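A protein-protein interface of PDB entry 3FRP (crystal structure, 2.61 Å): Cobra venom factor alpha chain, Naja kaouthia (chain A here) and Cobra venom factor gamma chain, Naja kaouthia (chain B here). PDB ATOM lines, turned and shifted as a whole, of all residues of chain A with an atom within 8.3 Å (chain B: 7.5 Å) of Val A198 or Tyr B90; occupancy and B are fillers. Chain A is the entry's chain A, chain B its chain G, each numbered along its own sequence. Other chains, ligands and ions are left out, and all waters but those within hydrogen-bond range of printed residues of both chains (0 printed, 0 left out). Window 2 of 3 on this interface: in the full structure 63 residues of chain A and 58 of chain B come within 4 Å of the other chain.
Tyr B90 touches Pro A117 (OH to CD, 3.4 Å). Lys A196 touches Tyr B90. Lys B21 touches Tyr A197 (CD to OH, 3.6 Å). N of Tyr A197 touches CD1 of Tyr B90 (3.7 Å). Met B88 touches Val A198. Val A198 touches Tyr B90 (CG1 to N, 3.9 Å). Leu A199 touches Lys B21. Pro A200 touches Gln B87. O of Ser A304 touches CG of Gln B87 (3.7 Å).
The backbone carbonyl oxygen of Leu A199 lies within hydrogen-bond range of the side-chain amide nitrogen of Gln B87, 3.1 Å away. The side-chain carboxylate (OD1) of Asp A305 lies within hydrogen-bond range of the side-chain amide nitrogen (NE2) of Gln B87, 3.0 Å away.
Of the 12 printed residues of chain B, 4 touch a printed residue of chain A. Printed residues of chain B that touch a printed residue of chain A: Lys B21, Gln B87, Met B88 and Tyr B90. Along chain A the printed residues that touch a printed residue of chain B span positions 117 to 305. Among the printed residues, 11 pairs touch across the chains.
O of Ile A114 is in hydrogen-bond range of OH of Tyr A197, at 3.0 Å. N of Ser A201 lies within hydrogen-bond range of OD1 of Asp A305 (3.0 Å).
Of chain A, only Pro A117, Lys A196, Tyr A197 and Val A198 come within 4 Å of Tyr B90. No residue of chain A comes within 4 Å of Ser B91. Of the printed residues of chain B, Tyr A197 touches Lys B21 and Tyr B90. Of the printed residues of chain A, Met B88 touches Val A198. Printed residues of chain B within 4 Å of Pro A117: Tyr B90. Printed residues of chain B within 4 Å of Asp A305: Gln B87. Printed residues of chain B within 4 Å of Pro A200: Gln B87. Met A306 touches none of the printed residues of chain B. The nearest residue of chain B that does not touch Val A198 is Pro B89 (4.1 Å). The nearest printed residue of chain B that does not touch Leu A199 is Met B88 (6.6 Å).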
ATOM      1  N   ILE A 114      11.315  -6.760  11.793  1.00  0.00           N
ATOM      2  CA  ILE A 114      11.278  -5.481  11.061  1.00  0.00           C
ATOM      3  C   ILE A 114      11.420  -4.208  11.952  1.00  0.00           C
ATOM      4  O   ILE A 114      10.740  -4.072  12.969  1.00  0.00           O
ATOM      5  CB  ILE A 114      10.048  -5.404  10.081  1.00  0.00           C
ATOM      6  CG1 ILE A 114      10.158  -4.196   9.140  1.00  0.00           C
ATOM      7  CG2 ILE A 114       8.703  -5.446  10.835  1.00  0.00           C
ATOM      8  CD1 ILE A 114       9.068  -4.140   8.082  1.00  0.00           C
ATOM      9  N   TYR A 115      12.323  -3.298  11.554  1.00  0.00           N
ATOM     10  CA  TYR A 115      12.618  -2.090  12.315  1.00  0.00           C
ATOM     11  C   TYR A 115      12.433  -0.824  11.481  1.00  0.00           C
ATOM     12  O   TYR A 115      12.412  -0.880  10.259  1.00  0.00           O
ATOM     13  CB  TYR A 115      14.025  -2.178  12.929  1.00  0.00           C
ATOM     14  CG  TYR A 115      14.199  -3.371  13.841  1.00  0.00           C
ATOM     15  CD1 TYR A 115      14.395  -4.659  13.317  1.00  0.00           C
ATOM     16  CD2 TYR A 115      14.135  -3.237  15.223  1.00  0.00           C
ATOM     17  CE1 TYR A 115      14.519  -5.791  14.164  1.00  0.00           C
ATOM     18  CE2 TYR A 115      14.264  -4.363  16.077  1.00  0.00           C
ATOM     19  CZ  TYR A 115      14.456  -5.626  15.530  1.00  0.00           C
ATOM     20  OH  TYR A 115      14.577  -6.727  16.340  1.00  0.00           O
ATOM     21  N   THR A 116      12.250   0.309  12.154  1.00  0.00           N
ATOM     22  CA  THR A 116      12.193   1.623  11.498  1.00  0.00           C
ATOM     23  C   THR A 116      13.555   2.287  11.697  1.00  0.00           C
ATOM     24  O   THR A 116      14.259   1.958  12.663  1.00  0.00           O
ATOM     25  CB  THR A 116      11.115   2.550  12.137  1.00  0.00           C
ATOM     26  OG1 THR A 116      11.203   2.498  13.569  1.00  0.00           O
ATOM     27  CG2 THR A 116       9.710   2.148  11.723  1.00  0.00           C
ATOM     28  N   PRO A 117      13.950   3.216  10.802  1.00  0.00           N
ATOM     29  CA  PRO A 117      15.225   3.876  11.067  1.00  0.00           C
ATOM     30  C   PRO A 117      15.201   4.543  12.451  1.00  0.00           C
ATOM     31  O   PRO A 117      14.147   5.006  12.909  1.00  0.00           O
ATOM     32  CB  PRO A 117      15.300   4.938   9.965  1.00  0.00           C
ATOM     33  CG  PRO A 117      14.336   4.494   8.923  1.00  0.00           C
ATOM     34  CD  PRO A 117      13.252   3.823   9.654  1.00  0.00           C
ATOM     35  N   GLY A 118      16.342   4.551  13.127  1.00  0.00           N
ATOM     36  CA  GLY A 118      16.433   5.148  14.460  1.00  0.00           C
ATOM     37  C   GLY A 118      15.676   4.423  15.559  1.00  0.00           C
ATOM     38  O   GLY A 118      15.020   5.067  16.385  1.00  0.00           O
ATOM     39  N   PRO A 167      20.815   3.940  13.112  1.00  0.00           N
ATOM     40  CA  PRO A 167      20.914   5.360  12.788  1.00  0.00           C
ATOM     41  C   PRO A 167      19.652   5.916  12.111  1.00  0.00           C
ATOM     42  O   PRO A 167      18.970   5.186  11.396  1.00  0.00           O
ATOM     43  CB  PRO A 167      22.102   5.418  11.817  1.00  0.00           C
ATOM     44  CG  PRO A 167      22.892   4.176  12.081  1.00  0.00           C
ATOM     45  CD  PRO A 167      21.890   3.148  12.483  1.00  0.00           C
ATOM     46  N   ASP A 168      19.374   7.203  12.346  1.00  0.00           N
ATOM     47  CA  ASP A 168      18.223   7.924  11.771  1.00  0.00           C
ATOM     48  C   ASP A 168      18.220   7.955  10.238  1.00  0.00           C
ATOM     49  O   ASP A 168      17.158   7.873   9.611  1.00  0.00           O
ATOM     50  CB  ASP A 168      18.142   9.360  12.323  1.00  0.00           C
ATOM     51  CG  ASP A 168      17.905   9.402  13.833  1.00  0.00           C
ATOM     52  OD1 ASP A 168      16.817   8.959  14.293  1.00  0.00           O
ATOM     53  OD2 ASP A 168      18.808   9.884  14.562  1.00  0.00           O
ATOM     54  N   LEU A 172      18.105   0.980   3.640  1.00  0.00           N
ATOM     55  CA  LEU A 172      16.881   0.243   3.858  1.00  0.00           C
ATOM     56  C   LEU A 172      16.916  -1.148   3.198  1.00  0.00           C
ATOM     57  O   LEU A 172      17.376  -1.309   2.064  1.00  0.00           O
ATOM     58  CB  LEU A 172      15.684   1.064   3.369  1.00  0.00           C
ATOM     59  CG  LEU A 172      15.623   2.518   3.862  1.00  0.00           C
ATOM     60  CD1 LEU A 172      14.464   3.287   3.202  1.00  0.00           C
ATOM     61  CD2 LEU A 172      15.545   2.605   5.391  1.00  0.00           C
ATOM     62  N   VAL A 194      14.861  -3.305   7.561  1.00  0.00           N
ATOM     63  CA  VAL A 194      14.729  -1.935   7.995  1.00  0.00           C
ATOM     64  C   VAL A 194      13.889  -1.204   6.953  1.00  0.00           C
ATOM     65  O   VAL A 194      14.324  -1.007   5.823  1.00  0.00           O
ATOM     66  CB  VAL A 194      16.111  -1.260   8.189  1.00  0.00           C
ATOM     67  CG1 VAL A 194      15.954   0.251   8.546  1.00  0.00           C
ATOM     68  CG2 VAL A 194      16.950  -1.997   9.267  1.00  0.00           C
ATOM     69  N   ARG A 195      12.670  -0.827   7.317  1.00  0.00           N
ATOM     70  CA  ARG A 195      11.785  -0.155   6.369  1.00  0.00           C
ATOM     71  C   ARG A 195      11.128   1.036   7.028  1.00  0.00           C
ATOM     72  O   ARG A 195      10.975   1.053   8.251  1.00  0.00           O
ATOM     73  CB  ARG A 195      10.704  -1.113   5.827  1.00  0.00           C
ATOM     74  CG  ARG A 195      11.220  -2.197   4.879  1.00  0.00           C
ATOM     75  CD  ARG A 195      10.129  -2.745   3.928  1.00  0.00           C
ATOM     76  NE  ARG A 195      10.352  -4.169   3.608  1.00  0.00           N
ATOM     77  CZ  ARG A 195       9.429  -5.136   3.708  1.00  0.00           C
ATOM     78  NH1 ARG A 195       8.182  -4.857   4.080  1.00  0.00           N
ATOM     79  NH2 ARG A 195       9.744  -6.393   3.408  1.00  0.00           N
ATOM     80  N   LYS A 196      10.744   2.024   6.219  1.00  0.00           N
ATOM     81  CA  LYS A 196       9.925   3.140   6.686  1.00  0.00           C
ATOM     82  C   LYS A 196       8.458   2.706   6.713  1.00  0.00           C
ATOM     83  O   LYS A 196       7.665   3.077   5.826  1.00  0.00           O
ATOM     84  CB  LYS A 196      10.087   4.376   5.788  1.00  0.00           C
ATOM     85  CG  LYS A 196      11.453   5.069   5.820  1.00  0.00           C
ATOM     86  CD  LYS A 196      11.386   6.394   5.034  1.00  0.00           C
ATOM     87  CE  LYS A 196      12.773   6.961   4.670  1.00  0.00           C
ATOM     88  NZ  LYS A 196      12.667   8.025   3.610  1.00  0.00           N
ATOM     89  N   TYR A 197       8.089   1.939   7.741  1.00  0.00           N
ATOM     90  CA  TYR A 197       6.745   1.348   7.814  1.00  0.00           C
ATOM     91  C   TYR A 197       5.895   1.729   9.039  1.00  0.00           C
ATOM     92  O   TYR A 197       6.414   1.997  10.121  1.00  0.00           O
ATOM     93  CB  TYR A 197       6.848  -0.173   7.746  1.00  0.00           C
ATOM     94  CG  TYR A 197       7.209  -0.801   9.078  1.00  0.00           C
ATOM     95  CD1 TYR A 197       6.237  -1.427   9.857  1.00  0.00           C
ATOM     96  CD2 TYR A 197       8.519  -0.766   9.564  1.00  0.00           C
ATOM     97  CE1 TYR A 197       6.558  -2.015  11.079  1.00  0.00           C
ATOM     98  CE2 TYR A 197       8.852  -1.351  10.798  1.00  0.00           C
ATOM     99  CZ  TYR A 197       7.864  -1.976  11.550  1.00  0.00           C
ATOM    100  OH  TYR A 197       8.172  -2.550  12.776  1.00  0.00           O
ATOM    101  N   VAL A 198       4.577   1.725   8.842  1.00  0.00           N
ATOM    102  CA  VAL A 198       3.610   1.738   9.940  1.00  0.00           C
ATOM    103  C   VAL A 198       2.956   0.367  10.062  1.00  0.00           C
ATOM    104  O   VAL A 198       2.621  -0.232   9.050  1.00  0.00           O
ATOM    105  CB  VAL A 198       2.503   2.793   9.712  1.00  0.00           C
ATOM    106  CG1 VAL A 198       2.962   4.155  10.202  1.00  0.00           C
ATOM    107  CG2 VAL A 198       2.056   2.840   8.209  1.00  0.00           C
ATOM    108  N   LEU A 199       2.786  -0.121  11.294  1.00  0.00           N
ATOM    109  CA  LEU A 199       2.018  -1.356  11.598  1.00  0.00           C
ATOM    110  C   LEU A 199       0.558  -1.302  11.122  1.00  0.00           C
ATOM    111  O   LEU A 199      -0.152  -0.337  11.394  1.00  0.00           O
ATOM    112  CB  LEU A 199       2.023  -1.625  13.101  1.00  0.00           C
ATOM    113  CG  LEU A 199       2.865  -2.733  13.739  1.00  0.00           C
ATOM    114  CD1 LEU A 199       4.282  -2.858  13.193  1.00  0.00           C
ATOM    115  CD2 LEU A 199       2.889  -2.498  15.260  1.00  0.00           C
ATOM    116  N   PRO A 200       0.096  -2.348  10.420  1.00  0.00           N
ATOM    117  CA  PRO A 200      -1.293  -2.344   9.970  1.00  0.00           C
ATOM    118  C   PRO A 200      -2.258  -2.822  11.085  1.00  0.00           C
ATOM    119  O   PRO A 200      -1.827  -3.521  12.004  1.00  0.00           O
ATOM    120  CB  PRO A 200      -1.261  -3.316   8.788  1.00  0.00           C
ATOM    121  CG  PRO A 200      -0.206  -4.320   9.167  1.00  0.00           C
ATOM    122  CD  PRO A 200       0.771  -3.625  10.114  1.00  0.00           C
ATOM    123  N   SER A 201      -3.539  -2.455  11.005  1.00  0.00           N
ATOM    124  CA  SER A 201      -4.515  -2.821  12.057  1.00  0.00           C
ATOM    125  C   SER A 201      -5.083  -4.232  11.928  1.00  0.00           C
ATOM    126  O   SER A 201      -5.748  -4.703  12.850  1.00  0.00           O
ATOM    127  CB  SER A 201      -5.670  -1.841  12.086  1.00  0.00           C
ATOM    128  OG  SER A 201      -6.321  -1.888  10.834  1.00  0.00           O
ATOM    129  N   SER A 304      -8.966   3.511   5.461  1.00  0.00           N
ATOM    130  CA  SER A 304      -7.963   3.830   6.516  1.00  0.00           C
ATOM    131  C   SER A 304      -6.573   3.175   6.345  1.00  0.00           C
ATOM    132  O   SER A 304      -5.552   3.838   6.524  1.00  0.00           O
ATOM    133  CB  SER A 304      -8.506   3.566   7.941  1.00  0.00           C
ATOM    134  OG  SER A 304      -9.083   2.269   8.096  1.00  0.00           O
ATOM    135  N   ASP A 305      -6.531   1.884   6.036  1.00  0.00           N
ATOM    136  CA  ASP A 305      -5.251   1.242   5.757  1.00  0.00           C
ATOM    137  C   ASP A 305      -5.421  -0.038   4.992  1.00  0.00           C
ATOM    138  O   ASP A 305      -6.513  -0.582   4.921  1.00  0.00           O
ATOM    139  CB  ASP A 305      -4.371   1.034   7.021  1.00  0.00           C
ATOM    140  CG  ASP A 305      -4.872  -0.074   7.937  1.00  0.00           C
ATOM    141  OD1 ASP A 305      -4.036  -0.697   8.634  1.00  0.00           O
ATOM    142  OD2 ASP A 305      -6.099  -0.322   7.975  1.00  0.00           O
ATOM    143  N   MET A 306      -4.317  -0.496   4.413  1.00  0.00           N
ATOM    144  CA  MET A 306      -4.283  -1.716   3.627  1.00  0.00           C
ATOM    145  C   MET A 306      -3.120  -2.639   4.015  1.00  0.00           C
ATOM    146  O   MET A 306      -2.222  -2.260   4.776  1.00  0.00           O
ATOM    147  CB  MET A 306      -4.242  -1.382   2.136  1.00  0.00           C
ATOM    148  CG  MET A 306      -2.897  -0.966   1.640  1.00  0.00           C
ATOM    149  SD  MET A 306      -3.013  -0.460  -0.074  1.00  0.00           S
ATOM    150  CE  MET A 306      -1.270  -0.085  -0.371  1.00  0.00           C
ATOM    151  N   VAL A 307      -3.169  -3.861   3.490  1.00  0.00           N
ATOM    152  CA  VAL A 307      -2.182  -4.889   3.783  1.00  0.00           C
ATOM    153  C   VAL A 307      -1.805  -5.589   2.473  1.00  0.00           C
ATOM    154  O   VAL A 307      -2.649  -5.778   1.589  1.00  0.00           O
ATOM    155  CB  VAL A 307      -2.715  -5.879   4.859  1.00  0.00           C
ATOM    156  CG1 VAL A 307      -1.813  -7.096   5.017  1.00  0.00           C
ATOM    157  CG2 VAL A 307      -2.852  -5.177   6.196  1.00  0.00           C
ATOM    158  N   ALA A 561       0.798  -7.416  15.309  1.00  0.00           N
ATOM    159  CA  ALA A 561       0.825  -6.687  14.061  1.00  0.00           C
ATOM    160  C   ALA A 561       2.203  -6.801  13.416  1.00  0.00           C
ATOM    161  O   ALA A 561       2.337  -6.609  12.203  1.00  0.00           O
ATOM    162  CB  ALA A 561       0.432  -5.240  14.274  1.00  0.00           C
ATOM    163  N   LEU A 565       3.536  -8.490   9.143  1.00  0.00           N
ATOM    164  CA  LEU A 565       4.471  -7.884   8.213  1.00  0.00           C
ATOM    165  C   LEU A 565       5.668  -8.779   7.818  1.00  0.00           C
ATOM    166  O   LEU A 565       6.170  -8.670   6.692  1.00  0.00           O
ATOM    167  CB  LEU A 565       4.931  -6.528   8.753  1.00  0.00           C
ATOM    168  CG  LEU A 565       3.930  -5.378   8.555  1.00  0.00           C
ATOM    169  CD1 LEU A 565       4.162  -4.309   9.617  1.00  0.00           C
ATOM    170  CD2 LEU A 565       3.948  -4.754   7.115  1.00  0.00           C
ATOM    171  N   LYS B  21       6.130  -1.540  20.124  1.00  0.00           N
ATOM    172  CA  LYS B  21       5.982  -2.612  19.165  1.00  0.00           C
ATOM    173  C   LYS B  21       6.521  -3.909  19.778  1.00  0.00           C
ATOM    174  O   LYS B  21       6.286  -4.995  19.258  1.00  0.00           O
ATOM    175  CB  LYS B  21       6.680  -2.279  17.853  1.00  0.00           C
ATOM    176  CG  LYS B  21       6.094  -1.117  17.050  1.00  0.00           C
ATOM    177  CD  LYS B  21       6.924  -0.993  15.740  1.00  0.00           C
ATOM    178  CE  LYS B  21       6.469   0.130  14.799  1.00  0.00           C
ATOM    179  NZ  LYS B  21       6.734   1.478  15.378  1.00  0.00           N
ATOM    180  N   GLN B  87      -4.995   5.586  12.531  1.00  0.00           N
ATOM    181  CA  GLN B  87      -4.015   5.091  11.587  1.00  0.00           C
ATOM    182  C   GLN B  87      -3.352   6.308  10.963  1.00  0.00           C
ATOM    183  O   GLN B  87      -4.009   7.116  10.299  1.00  0.00           O
ATOM    184  CB  GLN B  87      -4.707   4.234  10.522  1.00  0.00           C
ATOM    185  CG  GLN B  87      -3.829   3.236   9.785  1.00  0.00           C
ATOM    186  CD  GLN B  87      -3.307   2.089  10.653  1.00  0.00           C
ATOM    187  OE1 GLN B  87      -3.706   1.909  11.820  1.00  0.00           O
ATOM    188  NE2 GLN B  87      -2.390   1.309  10.079  1.00  0.00           N
ATOM    189  N   MET B  88      -2.045   6.415  11.195  1.00  0.00           N
ATOM    190  CA  MET B  88      -1.240   7.567  10.838  1.00  0.00           C
ATOM    191  C   MET B  88      -0.264   7.191   9.730  1.00  0.00           C
ATOM    192  O   MET B  88       0.218   6.070   9.713  1.00  0.00           O
ATOM    193  CB  MET B  88      -0.458   7.993  12.082  1.00  0.00           C
ATOM    194  CG  MET B  88      -1.336   8.378  13.303  1.00  0.00           C
ATOM    195  SD  MET B  88      -1.362  10.157  13.685  1.00  0.00           S
ATOM    196  CE  MET B  88      -2.264  10.850  12.319  1.00  0.00           C
ATOM    197  N   PRO B  89       0.045   8.114   8.801  1.00  0.00           N
ATOM    198  CA  PRO B  89       1.106   7.782   7.831  1.00  0.00           C
ATOM    199  C   PRO B  89       2.501   7.811   8.481  1.00  0.00           C
ATOM    200  O   PRO B  89       2.670   8.395   9.547  1.00  0.00           O
ATOM    201  CB  PRO B  89       0.986   8.877   6.760  1.00  0.00           C
ATOM    202  CG  PRO B  89      -0.250   9.669   7.118  1.00  0.00           C
ATOM    203  CD  PRO B  89      -0.485   9.467   8.586  1.00  0.00           C
ATOM    204  N   TYR B  90       3.487   7.172   7.853  1.00  0.00           N
ATOM    205  CA  TYR B  90       4.837   7.102   8.423  1.00  0.00           C
ATOM    206  C   TYR B  90       5.362   8.507   8.757  1.00  0.00           C
ATOM    207  O   TYR B  90       6.002   8.728   9.798  1.00  0.00           O
ATOM    208  CB  TYR B  90       5.808   6.387   7.462  1.00  0.00           C
ATOM    209  CG  TYR B  90       7.233   6.382   7.971  1.00  0.00           C
ATOM    210  CD1 TYR B  90       7.650   5.442   8.920  1.00  0.00           C
ATOM    211  CD2 TYR B  90       8.153   7.342   7.540  1.00  0.00           C
ATOM    212  CE1 TYR B  90       8.940   5.447   9.414  1.00  0.00           C
ATOM    213  CE2 TYR B  90       9.441   7.357   8.027  1.00  0.00           C
ATOM    214  CZ  TYR B  90       9.828   6.408   8.966  1.00  0.00           C
ATOM    215  OH  TYR B  90      11.114   6.403   9.456  1.00  0.00           O
ATOM    216  N   SER B  91       5.075   9.438   7.855  1.00  0.00           N
ATOM    217  CA  SER B  91       5.609  10.763   7.907  1.00  0.00           C
ATOM    218  C   SER B  91       4.755  11.630   6.995  1.00  0.00           C
ATOM    219  O   SER B  91       4.092  11.120   6.102  1.00  0.00           O
ATOM    220  CB  SER B  91       7.087  10.777   7.460  1.00  0.00           C
ATOM    221  OG  SER B  91       7.228  10.756   6.040  1.00  0.00           O
ATOM    222  N   VAL B  92       4.773  12.938   7.244  1.00  0.00           N
ATOM    223  CA  VAL B  92       4.079  13.932   6.418  1.00  0.00           C
ATOM    224  C   VAL B  92       4.996  15.133   6.151  1.00  0.00           C
ATOM    225  O   VAL B  92       5.920  15.393   6.917  1.00  0.00           O
ATOM    226  CB  VAL B  92       2.789  14.405   7.099  1.00  0.00           C
ATOM    227  CG1 VAL B  92       2.096  15.500   6.248  1.00  0.00           C
ATOM    228  CG2 VAL B  92       1.856  13.224   7.322  1.00  0.00           C
ATOM    229  N   LYS B 180       2.107  10.202  18.206  1.00  0.00           N
ATOM    230  CA  LYS B 180       3.040  11.207  17.686  1.00  0.00           C
ATOM    231  C   LYS B 180       3.106  11.169  16.157  1.00  0.00           C
ATOM    232  O   LYS B 180       3.326  10.105  15.589  1.00  0.00           O
ATOM    233  CB  LYS B 180       4.443  11.004  18.293  1.00  0.00           C
ATOM    234  CG  LYS B 180       4.546  11.297  19.811  1.00  0.00           C
ATOM    235  CD  LYS B 180       5.605  12.383  20.100  1.00  0.00           C
ATOM    236  CE  LYS B 180       5.653  12.818  21.580  1.00  0.00           C
ATOM    237  NZ  LYS B 180       6.262  11.778  22.475  1.00  0.00           N
ATOM    238  N   LEU B 181       2.895  12.314  15.496  1.00  0.00           N
ATOM    239  CA  LEU B 181       2.943  12.367  14.027  1.00  0.00           C
ATOM    240  C   LEU B 181       4.307  12.856  13.599  1.00  0.00           C
ATOM    241  O   LEU B 181       4.812  13.810  14.180  1.00  0.00           O
ATOM    242  CB  LEU B 181       1.856  13.284  13.460  1.00  0.00           C
ATOM    243  CG  LEU B 181       1.882  13.618  11.957  1.00  0.00           C
ATOM    244  CD1 LEU B 181       1.523  12.413  11.096  1.00  0.00           C
ATOM    245  CD2 LEU B 181       0.985  14.803  11.601  1.00  0.00           C
ATOM    246  N   LYS B 182       4.905  12.202  12.601  1.00  0.00           N
ATOM    247  CA  LYS B 182       6.225  12.606  12.095  1.00  0.00           C
ATOM    248  C   LYS B 182       6.096  13.623  10.976  1.00  0.00           C
ATOM    249  O   LYS B 182       5.483  13.339   9.948  1.00  0.00           O
ATOM    250  CB  LYS B 182       7.070  11.409  11.620  1.00  0.00           C
ATOM    251  CG  LYS B 182       8.548  11.762  11.434  1.00  0.00           C
ATOM    252  CD  LYS B 182       9.310  10.834  10.488  1.00  0.00           C
ATOM    253  CE  LYS B 182       9.882   9.597  11.182  1.00  0.00           C
ATOM    254  NZ  LYS B 182      11.008   9.886  12.128  1.00  0.00           N
ATOM    255  N   VAL B 183       6.688  14.803  11.183  1.00  0.00           N
ATOM    256  CA  VAL B 183       6.705  15.850  10.162  1.00  0.00           C
ATOM    257  C   VAL B 183       8.123  16.117   9.674  1.00  0.00           C
ATOM    258  O   VAL B 183       9.033  16.333  10.474  1.00  0.00           O
ATOM    259  CB  VAL B 183       6.104  17.166  10.673  1.00  0.00           C
ATOM    260  CG1 VAL B 183       6.060  18.202   9.543  1.00  0.00           C
ATOM    261  CG2 VAL B 183       4.717  16.935  11.258  1.00  0.00           C
ATOM    262  N   VAL B 184       8.267  16.150   8.351  1.00  0.00           N
ATOM    263  CA  VAL B 184       9.553  16.184   7.662  1.00  0.00           C
ATOM    264  C   VAL B 184       9.703  17.444   6.785  1.00  0.00           C
ATOM    265  O   VAL B 184       8.709  17.968   6.294  1.00  0.00           O
ATOM    266  CB  VAL B 184       9.703  14.881   6.825  1.00  0.00           C
ATOM    267  CG1 VAL B 184      10.595  15.071   5.625  1.00  0.00           C
ATOM    268  CG2 VAL B 184      10.209  13.735   7.707  1.00  0.00           C
